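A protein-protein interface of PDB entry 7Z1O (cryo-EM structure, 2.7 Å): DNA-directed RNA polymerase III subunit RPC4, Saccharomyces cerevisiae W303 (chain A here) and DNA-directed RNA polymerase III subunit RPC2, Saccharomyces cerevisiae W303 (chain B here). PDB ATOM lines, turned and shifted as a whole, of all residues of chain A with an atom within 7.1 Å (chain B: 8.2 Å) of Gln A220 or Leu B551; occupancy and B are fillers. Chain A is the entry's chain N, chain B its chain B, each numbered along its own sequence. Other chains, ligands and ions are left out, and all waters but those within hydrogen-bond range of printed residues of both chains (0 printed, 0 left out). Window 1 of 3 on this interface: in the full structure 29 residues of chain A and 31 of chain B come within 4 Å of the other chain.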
ATOM      1  N   VAL A 212       0.260   7.332  21.916  1.00  0.00           N
ATOM      2  CA  VAL A 212       1.047   6.690  20.866  1.00  0.00           C
ATOM      3  C   VAL A 212       2.455   6.375  21.366  1.00  0.00           C
ATOM      4  O   VAL A 212       3.103   5.438  20.884  1.00  0.00           O
ATOM      5  CB  VAL A 212       1.059   7.568  19.597  1.00  0.00           C
ATOM      6  CG1 VAL A 212       1.839   8.859  19.821  1.00  0.00           C
ATOM      7  CG2 VAL A 212       1.603   6.795  18.401  1.00  0.00           C
ATOM      8  N   VAL A 215       2.112   3.174  24.285  1.00  0.00           N
ATOM      9  CA  VAL A 215       1.731   1.842  23.819  1.00  0.00           C
ATOM     10  C   VAL A 215       2.881   1.110  23.144  1.00  0.00           C
ATOM     11  O   VAL A 215       2.819  -0.118  22.994  1.00  0.00           O
ATOM     12  CB  VAL A 215       0.531   1.973  22.859  1.00  0.00           C
ATOM     13  CG1 VAL A 215       0.951   2.668  21.568  1.00  0.00           C
ATOM     14  CG2 VAL A 215      -0.170   0.634  22.607  1.00  0.00           C
ATOM     15  N   LYS A 216       3.948   1.826  22.767  1.00  0.00           N
ATOM     16  CA  LYS A 216       5.022   1.233  21.971  1.00  0.00           C
ATOM     17  C   LYS A 216       5.715   0.099  22.716  1.00  0.00           C
ATOM     18  O   LYS A 216       6.140  -0.888  22.100  1.00  0.00           O
ATOM     19  CB  LYS A 216       6.032   2.311  21.579  1.00  0.00           C
ATOM     20  CG  LYS A 216       5.563   3.214  20.453  1.00  0.00           C
ATOM     21  CD  LYS A 216       6.564   4.323  20.177  1.00  0.00           C
ATOM     22  CE  LYS A 216       6.225   5.062  18.894  1.00  0.00           C
ATOM     23  NZ  LYS A 216       6.293   6.538  19.072  1.00  0.00           N
ATOM     24  N   ARG A 217       5.833   0.220  24.041  1.00  0.00           N
ATOM     25  CA  ARG A 217       6.417  -0.854  24.839  1.00  0.00           C
ATOM     26  C   ARG A 217       5.574  -2.120  24.756  1.00  0.00           C
ATOM     27  O   ARG A 217       6.107  -3.232  24.671  1.00  0.00           O
ATOM     28  CB  ARG A 217       6.573  -0.400  26.291  1.00  0.00           C
ATOM     29  CG  ARG A 217       7.314  -1.388  27.181  1.00  0.00           C
ATOM     30  CD  ARG A 217       8.810  -1.355  26.914  1.00  0.00           C
ATOM     31  NE  ARG A 217       9.207  -2.325  25.900  1.00  0.00           N
ATOM     32  CZ  ARG A 217      10.343  -2.275  25.220  1.00  0.00           C
ATOM     33  NH1 ARG A 217      11.223  -1.307  25.416  1.00  0.00           N
ATOM     34  NH2 ARG A 217      10.600  -3.216  24.316  1.00  0.00           N
ATOM     35  N   GLU A 218       4.248  -1.970  24.781  1.00  0.00           N
ATOM     36  CA  GLU A 218       3.369  -3.126  24.640  1.00  0.00           C
ATOM     37  C   GLU A 218       3.408  -3.680  23.220  1.00  0.00           C
ATOM     38  O   GLU A 218       3.391  -4.901  23.021  1.00  0.00           O
ATOM     39  CB  GLU A 218       1.941  -2.748  25.032  1.00  0.00           C
ATOM     40  CG  GLU A 218       0.941  -3.890  24.939  1.00  0.00           C
ATOM     41  CD  GLU A 218      -0.392  -3.552  25.576  1.00  0.00           C
ATOM     42  OE1 GLU A 218      -0.575  -2.388  25.993  1.00  0.00           O
ATOM     43  OE2 GLU A 218      -1.257  -4.449  25.660  1.00  0.00           O
ATOM     44  N   ILE A 219       3.470  -2.795  22.220  1.00  0.00           N
ATOM     45  CA  ILE A 219       3.399  -3.224  20.824  1.00  0.00           C
ATOM     46  C   ILE A 219       4.657  -3.988  20.427  1.00  0.00           C
ATOM     47  O   ILE A 219       4.590  -4.987  19.696  1.00  0.00           O
ATOM     48  CB  ILE A 219       3.155  -2.004  19.915  1.00  0.00           C
ATOM     49  CG1 ILE A 219       1.776  -1.409  20.202  1.00  0.00           C
ATOM     50  CG2 ILE A 219       3.264  -2.383  18.446  1.00  0.00           C
ATOM     51  CD1 ILE A 219       1.397  -0.277  19.290  1.00  0.00           C
ATOM     52  N   GLN A 220       5.822  -3.537  20.901  1.00  0.00           N
ATOM     53  CA  GLN A 220       7.071  -4.216  20.565  1.00  0.00           C
ATOM     54  C   GLN A 220       7.094  -5.640  21.111  1.00  0.00           C
ATOM     55  O   GLN A 220       7.631  -6.550  20.468  1.00  0.00           O
ATOM     56  CB  GLN A 220       8.263  -3.417  21.089  1.00  0.00           C
ATOM     57  CG  GLN A 220       8.553  -2.154  20.293  1.00  0.00           C
ATOM     58  CD  GLN A 220       9.722  -1.368  20.850  1.00  0.00           C
ATOM     59  OE1 GLN A 220      10.280  -1.715  21.891  1.00  0.00           O
ATOM     60  NE2 GLN A 220      10.099  -0.299  20.158  1.00  0.00           N
ATOM     61  N   GLU A 221       6.516  -5.853  22.295  1.00  0.00           N
ATOM     62  CA  GLU A 221       6.415  -7.208  22.827  1.00  0.00           C
ATOM     63  C   GLU A 221       5.315  -8.006  22.136  1.00  0.00           C
ATOM     64  O   GLU A 221       5.445  -9.224  21.973  1.00  0.00           O
ATOM     65  CB  GLU A 221       6.171  -7.165  24.336  1.00  0.00           C
ATOM     66  CG  GLU A 221       7.158  -6.301  25.116  1.00  0.00           C
ATOM     67  CD  GLU A 221       8.608  -6.551  24.738  1.00  0.00           C
ATOM     68  OE1 GLU A 221       9.014  -7.730  24.646  1.00  0.00           O
ATOM     69  OE2 GLU A 221       9.345  -5.564  24.531  1.00  0.00           O
ATOM     70  N   ALA A 222       4.233  -7.347  21.724  1.00  0.00           N
ATOM     71  CA  ALA A 222       3.111  -8.016  21.082  1.00  0.00           C
ATOM     72  C   ALA A 222       3.410  -8.439  19.649  1.00  0.00           C
ATOM     73  O   ALA A 222       2.732  -9.328  19.125  1.00  0.00           O
ATOM     74  CB  ALA A 222       1.875  -7.112  21.106  1.00  0.00           C
ATOM     75  N   LEU A 223       4.403  -7.827  19.006  1.00  0.00           N
ATOM     76  CA  LEU A 223       4.799  -8.211  17.657  1.00  0.00           C
ATOM     77  C   LEU A 223       5.715  -9.430  17.634  1.00  0.00           C
ATOM     78  O   LEU A 223       6.210  -9.801  16.566  1.00  0.00           O
ATOM     79  CB  LEU A 223       5.478  -7.040  16.944  1.00  0.00           C
ATOM     80  CG  LEU A 223       4.595  -5.840  16.602  1.00  0.00           C
ATOM     81  CD1 LEU A 223       5.402  -4.779  15.877  1.00  0.00           C
ATOM     82  CD2 LEU A 223       3.392  -6.271  15.777  1.00  0.00           C
ATOM     83  N   SER A 224       5.952 -10.058  18.784  1.00  0.00           N
ATOM     84  CA  SER A 224       6.756 -11.267  18.871  1.00  0.00           C
ATOM     85  C   SER A 224       5.964 -12.343  19.599  1.00  0.00           C
ATOM     86  O   SER A 224       5.027 -12.047  20.345  1.00  0.00           O
ATOM     87  CB  SER A 224       8.084 -11.013  19.595  1.00  0.00           C
ATOM     88  OG  SER A 224       7.891 -10.923  20.996  1.00  0.00           O
ATOM     89  N   LEU A 282      16.134  -1.970  28.286  1.00  0.00           N
ATOM     90  CA  LEU A 282      15.718  -2.604  27.041  1.00  0.00           C
ATOM     91  C   LEU A 282      16.815  -3.509  26.490  1.00  0.00           C
ATOM     92  O   LEU A 282      16.528  -4.575  25.937  1.00  0.00           O
ATOM     93  CB  LEU A 282      15.321  -1.537  26.020  1.00  0.00           C
ATOM     94  CG  LEU A 282      15.073  -1.959  24.571  1.00  0.00           C
ATOM     95  CD1 LEU A 282      13.984  -3.013  24.492  1.00  0.00           C
ATOM     96  CD2 LEU A 282      14.705  -0.750  23.729  1.00  0.00           C
ATOM     97  N   ASP A 286      16.536  -7.439  25.800  1.00  0.00           N
ATOM     98  CA  ASP A 286      16.887  -7.993  24.498  1.00  0.00           C
ATOM     99  C   ASP A 286      17.935  -9.088  24.623  1.00  0.00           C
ATOM    100  O   ASP A 286      17.887 -10.078  23.891  1.00  0.00           O
ATOM    101  CB  ASP A 286      17.376  -6.885  23.565  1.00  0.00           C
ATOM    102  CG  ASP A 286      16.270  -5.930  23.163  1.00  0.00           C
ATOM    103  OD1 ASP A 286      15.086  -6.318  23.252  1.00  0.00           O
ATOM    104  OD2 ASP A 286      16.583  -4.792  22.756  1.00  0.00           O
ATOM    105  N   LYS A 384      18.731  -6.853  19.653  1.00  0.00           N
ATOM    106  CA  LYS A 384      17.630  -7.555  19.006  1.00  0.00           C
ATOM    107  C   LYS A 384      17.199  -6.913  17.692  1.00  0.00           C
ATOM    108  O   LYS A 384      16.427  -7.522  16.945  1.00  0.00           O
ATOM    109  CB  LYS A 384      16.429  -7.642  19.962  1.00  0.00           C
ATOM    110  CG  LYS A 384      15.440  -8.760  19.643  1.00  0.00           C
ATOM    111  CD  LYS A 384      14.425  -8.957  20.753  1.00  0.00           C
ATOM    112  CE  LYS A 384      13.317  -9.899  20.312  1.00  0.00           C
ATOM    113  NZ  LYS A 384      12.540 -10.433  21.463  1.00  0.00           N
ATOM    114  N   GLU A 387      11.963  -4.920  14.880  1.00  0.00           N
ATOM    115  CA  GLU A 387      10.929  -5.946  14.924  1.00  0.00           C
ATOM    116  C   GLU A 387      10.180  -5.940  13.598  1.00  0.00           C
ATOM    117  O   GLU A 387       9.750  -4.881  13.129  1.00  0.00           O
ATOM    118  CB  GLU A 387       9.967  -5.704  16.088  1.00  0.00           C
ATOM    119  CG  GLU A 387      10.646  -5.544  17.438  1.00  0.00           C
ATOM    120  CD  GLU A 387      11.360  -6.803  17.890  1.00  0.00           C
ATOM    121  OE1 GLU A 387      10.860  -7.911  17.601  1.00  0.00           O
ATOM    122  OE2 GLU A 387      12.423  -6.685  18.534  1.00  0.00           O
ATOM    123  N   THR A 389       7.003  -7.415  11.319  1.00  0.00           N
ATOM    124  CA  THR A 389       5.703  -8.077  11.358  1.00  0.00           C
ATOM    125  C   THR A 389       5.481  -8.954  10.135  1.00  0.00           C
ATOM    126  O   THR A 389       4.621  -9.842  10.157  1.00  0.00           O
ATOM    127  CB  THR A 389       4.584  -7.043  11.462  1.00  0.00           C
ATOM    128  OG1 THR A 389       4.333  -6.481  10.167  1.00  0.00           O
ATOM    129  CG2 THR A 389       4.977  -5.932  12.413  1.00  0.00           C
ATOM    130  N   GLN B 270       0.747   3.099   6.431  1.00  0.00           N
ATOM    131  CA  GLN B 270       1.657   2.778   7.526  1.00  0.00           C
ATOM    132  C   GLN B 270       2.913   3.639   7.479  1.00  0.00           C
ATOM    133  O   GLN B 270       3.452   4.014   8.525  1.00  0.00           O
ATOM    134  CB  GLN B 270       2.024   1.297   7.483  1.00  0.00           C
ATOM    135  CG  GLN B 270       1.022   0.386   8.162  1.00  0.00           C
ATOM    136  CD  GLN B 270       1.102  -1.038   7.657  1.00  0.00           C
ATOM    137  OE1 GLN B 270       1.462  -1.280   6.506  1.00  0.00           O
ATOM    138  NE2 GLN B 270       0.770  -1.992   8.519  1.00  0.00           N
ATOM    139  N   GLY B 274       1.320   5.529  10.311  1.00  0.00           N
ATOM    140  CA  GLY B 274       1.806   4.619  11.333  1.00  0.00           C
ATOM    141  C   GLY B 274       0.665   4.090  12.177  1.00  0.00           C
ATOM    142  O   GLY B 274      -0.327   3.592  11.645  1.00  0.00           O
ATOM    143  N   ASN B 275       0.808   4.199  13.493  1.00  0.00           N
ATOM    144  CA  ASN B 275      -0.184   3.689  14.425  1.00  0.00           C
ATOM    145  C   ASN B 275      -1.073   4.777  15.012  1.00  0.00           C
ATOM    146  O   ASN B 275      -1.852   4.492  15.925  1.00  0.00           O
ATOM    147  CB  ASN B 275       0.510   2.926  15.556  1.00  0.00           C
ATOM    148  CG  ASN B 275       0.767   1.480  15.201  1.00  0.00           C
ATOM    149  OD1 ASN B 275       1.044   1.153  14.048  1.00  0.00           O
ATOM    150  ND2 ASN B 275       0.676   0.604  16.190  1.00  0.00           N
ATOM    151  N   ARG B 354       4.393  12.614   5.663  1.00  0.00           N
ATOM    152  CA  ARG B 354       4.194  12.487   7.102  1.00  0.00           C
ATOM    153  C   ARG B 354       4.399  13.821   7.808  1.00  0.00           C
ATOM    154  O   ARG B 354       3.648  14.167   8.728  1.00  0.00           O
ATOM    155  CB  ARG B 354       5.139  11.430   7.672  1.00  0.00           C
ATOM    156  CG  ARG B 354       5.088  11.307   9.183  1.00  0.00           C
ATOM    157  CD  ARG B 354       5.799  10.055   9.658  1.00  0.00           C
ATOM    158  NE  ARG B 354       5.775   9.923  11.109  1.00  0.00           N
ATOM    159  CZ  ARG B 354       4.761   9.425  11.802  1.00  0.00           C
ATOM    160  NH1 ARG B 354       3.659   9.000  11.205  1.00  0.00           N
ATOM    161  NH2 ARG B 354       4.854   9.350  13.126  1.00  0.00           N
ATOM    162  N   ASP B 545      10.708  -3.321   8.022  1.00  0.00           N
ATOM    163  CA  ASP B 545       9.263  -3.288   7.858  1.00  0.00           C
ATOM    164  C   ASP B 545       8.773  -1.859   7.694  1.00  0.00           C
ATOM    165  O   ASP B 545       9.267  -0.933   8.344  1.00  0.00           O
ATOM    166  CB  ASP B 545       8.574  -3.931   9.061  1.00  0.00           C
ATOM    167  CG  ASP B 545       7.129  -4.307   8.778  1.00  0.00           C
ATOM    168  OD1 ASP B 545       6.637  -4.027   7.664  1.00  0.00           O
ATOM    169  OD2 ASP B 545       6.481  -4.884   9.675  1.00  0.00           O
ATOM    170  N   SER B 546       7.788  -1.684   6.814  1.00  0.00           N
ATOM    171  CA  SER B 546       7.100  -0.405   6.728  1.00  0.00           C
ATOM    172  C   SER B 546       6.121  -0.223   7.881  1.00  0.00           C
ATOM    173  O   SER B 546       5.829   0.913   8.271  1.00  0.00           O
ATOM    174  CB  SER B 546       6.375  -0.294   5.393  1.00  0.00           C
ATOM    175  OG  SER B 546       7.251  -0.579   4.317  1.00  0.00           O
ATOM    176  N   ALA B 547       5.608  -1.326   8.431  1.00  0.00           N
ATOM    177  CA  ALA B 547       4.651  -1.235   9.529  1.00  0.00           C
ATOM    178  C   ALA B 547       5.322  -0.774  10.817  1.00  0.00           C
ATOM    179  O   ALA B 547       4.750   0.024  11.569  1.00  0.00           O
ATOM    180  CB  ALA B 547       3.962  -2.582   9.736  1.00  0.00           C
ATOM    181  N   SER B 548       6.531  -1.262  11.090  1.00  0.00           N
ATOM    182  CA  SER B 548       7.251  -0.936  12.315  1.00  0.00           C
ATOM    183  C   SER B 548       8.352   0.093  12.085  1.00  0.00           C
ATOM    184  O   SER B 548       9.346   0.112  12.818  1.00  0.00           O
ATOM    185  CB  SER B 548       7.833  -2.201  12.942  1.00  0.00           C
ATOM    186  OG  SER B 548       8.845  -2.756  12.123  1.00  0.00           O
ATOM    187  N   LEU B 549       8.199   0.945  11.070  1.00  0.00           N
ATOM    188  CA  LEU B 549       9.191   1.986  10.825  1.00  0.00           C
ATOM    189  C   LEU B 549       9.148   3.059  11.906  1.00  0.00           C
ATOM    190  O   LEU B 549      10.195   3.540  12.353  1.00  0.00           O
ATOM    191  CB  LEU B 549       8.968   2.612   9.450  1.00  0.00           C
ATOM    192  CG  LEU B 549       9.972   3.691   9.049  1.00  0.00           C
ATOM    193  CD1 LEU B 549      11.324   3.079   8.729  1.00  0.00           C
ATOM    194  CD2 LEU B 549       9.458   4.516   7.889  1.00  0.00           C
ATOM    195  N   HIS B 550       7.949   3.439  12.343  1.00  0.00           N
ATOM    196  CA  HIS B 550       7.770   4.508  13.316  1.00  0.00           C
ATOM    197  C   HIS B 550       7.725   4.001  14.750  1.00  0.00           C
ATOM    198  O   HIS B 550       7.521   4.797  15.671  1.00  0.00           O
ATOM    199  CB  HIS B 550       6.504   5.301  12.999  1.00  0.00           C
ATOM    200  CG  HIS B 550       6.418   5.751  11.575  1.00  0.00           C
ATOM    201  ND1 HIS B 550       7.396   6.515  10.977  1.00  0.00           N
ATOM    202  CD2 HIS B 550       5.473   5.543  10.629  1.00  0.00           C
ATOM    203  CE1 HIS B 550       7.057   6.759   9.724  1.00  0.00           C
ATOM    204  NE2 HIS B 550       5.894   6.180   9.487  1.00  0.00           N
ATOM    205  N   LEU B 551       7.904   2.699  14.962  1.00  0.00           N
ATOM    206  CA  LEU B 551       8.017   2.167  16.312  1.00  0.00           C
ATOM    207  C   LEU B 551       9.415   2.326  16.888  1.00  0.00           C
ATOM    208  O   LEU B 551       9.618   2.035  18.071  1.00  0.00           O
ATOM    209  CB  LEU B 551       7.620   0.690  16.332  1.00  0.00           C
ATOM    210  CG  LEU B 551       6.162   0.389  15.986  1.00  0.00           C
ATOM    211  CD1 LEU B 551       5.906  -1.104  16.039  1.00  0.00           C
ATOM    212  CD2 LEU B 551       5.224   1.132  16.922  1.00  0.00           C
ATOM    213  N   ASN B 552      10.376   2.777  16.086  1.00  0.00           N
ATOM    214  CA  ASN B 552      11.737   2.980  16.551  1.00  0.00           C
ATOM    215  C   ASN B 552      12.335   4.169  15.815  1.00  0.00           C
ATOM    216  O   ASN B 552      11.822   4.607  14.782  1.00  0.00           O
ATOM    217  CB  ASN B 552      12.591   1.720  16.360  1.00  0.00           C
ATOM    218  CG  ASN B 552      12.457   1.127  14.973  1.00  0.00           C
ATOM    219  OD1 ASN B 552      11.780   1.682  14.108  1.00  0.00           O
ATOM    220  ND2 ASN B 552      13.103  -0.012  14.755  1.00  0.00           N
ATOM    221  N   TYR B 553      13.423   4.692  16.374  1.00  0.00           N
ATOM    222  CA  TYR B 553      14.047   5.898  15.846  1.00  0.00           C
ATOM    223  C   TYR B 553      14.622   5.661  14.456  1.00  0.00           C
ATOM    224  O   TYR B 553      15.151   4.587  14.157  1.00  0.00           O
ATOM    225  CB  TYR B 553      15.149   6.364  16.797  1.00  0.00           C
ATOM    226  CG  TYR B 553      14.678   7.276  17.904  1.00  0.00           C
ATOM    227  CD1 TYR B 553      14.067   6.763  19.040  1.00  0.00           C
ATOM    228  CD2 TYR B 553      14.879   8.647  17.833  1.00  0.00           C
ATOM    229  CE1 TYR B 553      13.647   7.591  20.060  1.00  0.00           C
ATOM    230  CE2 TYR B 553      14.465   9.481  18.850  1.00  0.00           C
ATOM    231  CZ  TYR B 553      13.850   8.949  19.960  1.00  0.00           C
ATOM    232  OH  TYR B 553      13.434   9.778  20.976  1.00  0.00           O
ATOM    233  N   GLY B 554      14.507   6.673  13.599  1.00  0.00           N
ATOM    234  CA  GLY B 554      15.107   6.644  12.287  1.00  0.00           C
ATOM    235  C   GLY B 554      16.408   7.422  12.256  1.00  0.00           C
ATOM    236  O   GLY B 554      16.660   8.279  13.097  1.00  0.00           O
ATOM    237  N   SER B 564      16.918   2.594  10.251  1.00  0.00           N
ATOM    238  CA  SER B 564      16.365   2.675  11.595  1.00  0.00           C
ATOM    239  C   SER B 564      17.379   2.161  12.604  1.00  0.00           C
ATOM    240  O   SER B 564      18.179   1.274  12.294  1.00  0.00           O
ATOM    241  CB  SER B 564      15.064   1.874  11.709  1.00  0.00           C
ATOM    242  OG  SER B 564      15.322   0.483  11.725  1.00  0.00           O
ATOM    243  N   ILE B 565      17.338   2.718  13.813  1.00  0.00           N
ATOM    244  CA  ILE B 565      18.245   2.345  14.891  1.00  0.00           C
ATOM    245  C   ILE B 565      17.408   1.939  16.098  1.00  0.00           C
ATOM    246  O   ILE B 565      16.367   2.547  16.374  1.00  0.00           O
ATOM    247  CB  ILE B 565      19.228   3.484  15.235  1.00  0.00           C
ATOM    248  CG1 ILE B 565      20.238   3.038  16.293  1.00  0.00           C
ATOM    249  CG2 ILE B 565      18.497   4.746  15.682  1.00  0.00           C
ATOM    250  CD1 ILE B 565      21.181   1.959  15.817  1.00  0.00           C
ATOM    251  N   ARG B 566      17.837   0.879  16.784  1.00  0.00           N
ATOM    252  CA  ARG B 566      17.098   0.408  17.950  1.00  0.00           C
ATOM    253  C   ARG B 566      17.433   1.237  19.186  1.00  0.00           C
ATOM    254  O   ARG B 566      16.543   1.568  19.978  1.00  0.00           O
ATOM    255  CB  ARG B 566      17.398  -1.071  18.188  1.00  0.00           C
ATOM    256  CG  ARG B 566      16.662  -1.690  19.359  1.00  0.00           C
ATOM    257  CD  ARG B 566      15.175  -1.756  19.075  1.00  0.00           C
ATOM    258  NE  ARG B 566      14.429  -2.356  20.173  1.00  0.00           N
ATOM    259  CZ  ARG B 566      14.183  -3.655  20.283  1.00  0.00           C
ATOM    260  NH1 ARG B 566      14.617  -4.519  19.382  1.00  0.00           N
ATOM    261  NH2 ARG B 566      13.482  -4.096  21.323  1.00  0.00           N
ATOM    262  N   PHE B 567      18.708   1.587  19.363  1.00  0.00           N
ATOM    263  CA  PHE B 567      19.162   2.386  20.498  1.00  0.00           C
ATOM    264  C   PHE B 567      19.712   3.715  19.998  1.00  0.00           C
ATOM    265  O   PHE B 567      20.864   3.776  19.543  1.00  0.00           O
ATOM    266  CB  PHE B 567      20.230   1.633  21.295  1.00  0.00           C
ATOM    267  CG  PHE B 567      19.806   0.265  21.740  1.00  0.00           C
ATOM    268  CD1 PHE B 567      18.535   0.046  22.241  1.00  0.00           C
ATOM    269  CD2 PHE B 567      20.679  -0.805  21.652  1.00  0.00           C
ATOM    270  CE1 PHE B 567      18.145  -1.213  22.650  1.00  0.00           C
ATOM    271  CE2 PHE B 567      20.294  -2.066  22.060  1.00  0.00           C
ATOM    272  CZ  PHE B 567      19.026  -2.271  22.558  1.00  0.00           C
ATOM    273  N   MET B 597      11.245  11.732  16.329  1.00  0.00           N
ATOM    274  CA  MET B 597      11.826  10.407  16.547  1.00  0.00           C
ATOM    275  C   MET B 597      12.864  10.082  15.475  1.00  0.00           C
ATOM    276  O   MET B 597      12.714   9.156  14.677  1.00  0.00           O
ATOM    277  CB  MET B 597      10.748   9.322  16.616  1.00  0.00           C
ATOM    278  CG  MET B 597       9.832   9.421  17.818  1.00  0.00           C
ATOM    279  SD  MET B 597       8.550   8.159  17.777  1.00  0.00           S
ATOM    280  CE  MET B 597       9.527   6.693  18.103  1.00  0.00           C
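NH2 of Arg A217 is in hydrogen-bond range of OE1 of Gln A220, at 2.9 Å.
O of Gln B270 sits close to NE2 of His B550 (3.4 Å).
OD1 of Asp B545 sits at hydrogen-bond distance from N of Ala B547, 3.0 Å away.
The backbone carbonyl oxygen (O) of Ser B548 lies close to the side-chain amide oxygen (OD1) of Asn B552 (3.2 Å).
The backbone carbonyl oxygen (O) of Met B597 is in hydrogen-bond range of the backbone NH (N) of Gly B554, at 3.2 Å.
Gln A220 touches just one residue of chain B: Leu B551.
Of the printed residues of chain B, Glu A387 touches Ser B548 (2.5 Å) and Arg B566 (3.2 Å).
Of the printed residues of chain A, Asp B545 touches Thr A389 (2.7 Å).
Of chain A, only Ile A219, Gln A220 and Leu A223 come within 4 Å of Leu B551.
Printed residues of chain A within 4 Å of Met B597: Lys A216 (3.1 Å).
The nearest residue of chain A that does not touch Leu B551 is Lys A216 (4.1 Å).
The nearest printed residue of chain A that does not touch Phe B567 is Lys A384 (5.4 Å).
Among the printed residues, merely in contact across the chains: Ile A219 with Asn B275 (3.3 Å), Leu A282 with Arg B566 (3.4 Å), Lys A216 with His B550 (3.5 Å), Asp A286 with Phe B567 (3.5 Å), Leu A282 with Phe B567 (3.6 Å), Lys A384 with Arg B566 (3.7 Å), Leu A223 with Leu B551 (3.7 Å), Ile A219 with Leu B551 (3.8 Å) and Thr A389 with Ala B547 (3.9 Å).
Hydrophobic or aromatic side chains of chain A that line the printed part of chain B: Ile A219, Leu A223 and Leu A282.
Of the 19 printed residues of chain B, 9 touch a printed residue of chain A.
Among the printed residues, Asp or Glu carboxylates within 4 Å of a Lys or Arg side-chain nitrogen of the other chain: Asp A286 with Arg B566 (3.4 Å) and Glu A387 with Arg B566 (3.2 Å).
SD of Met B597 is in hydrogen-bond range of NZ of Lys A216 (3.1 Å).
O of Leu B551 sits at hydrogen-bond distance from NE2 of Gln A220, at 3.2 Å.
OD1 of Asp A286 is in salt-bridge range of NH2 of Arg B566 (3.4 Å).
O of Glu A387 sits at hydrogen-bond distance from OG of Ser B548, 2.5 Å away.
NH1 of Arg B566 lies within salt-bridge range of OE2 of Glu A387 (3.2 Å).
OG1 of Thr A389 sits at hydrogen-bond distance from OD2 of Asp B545.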
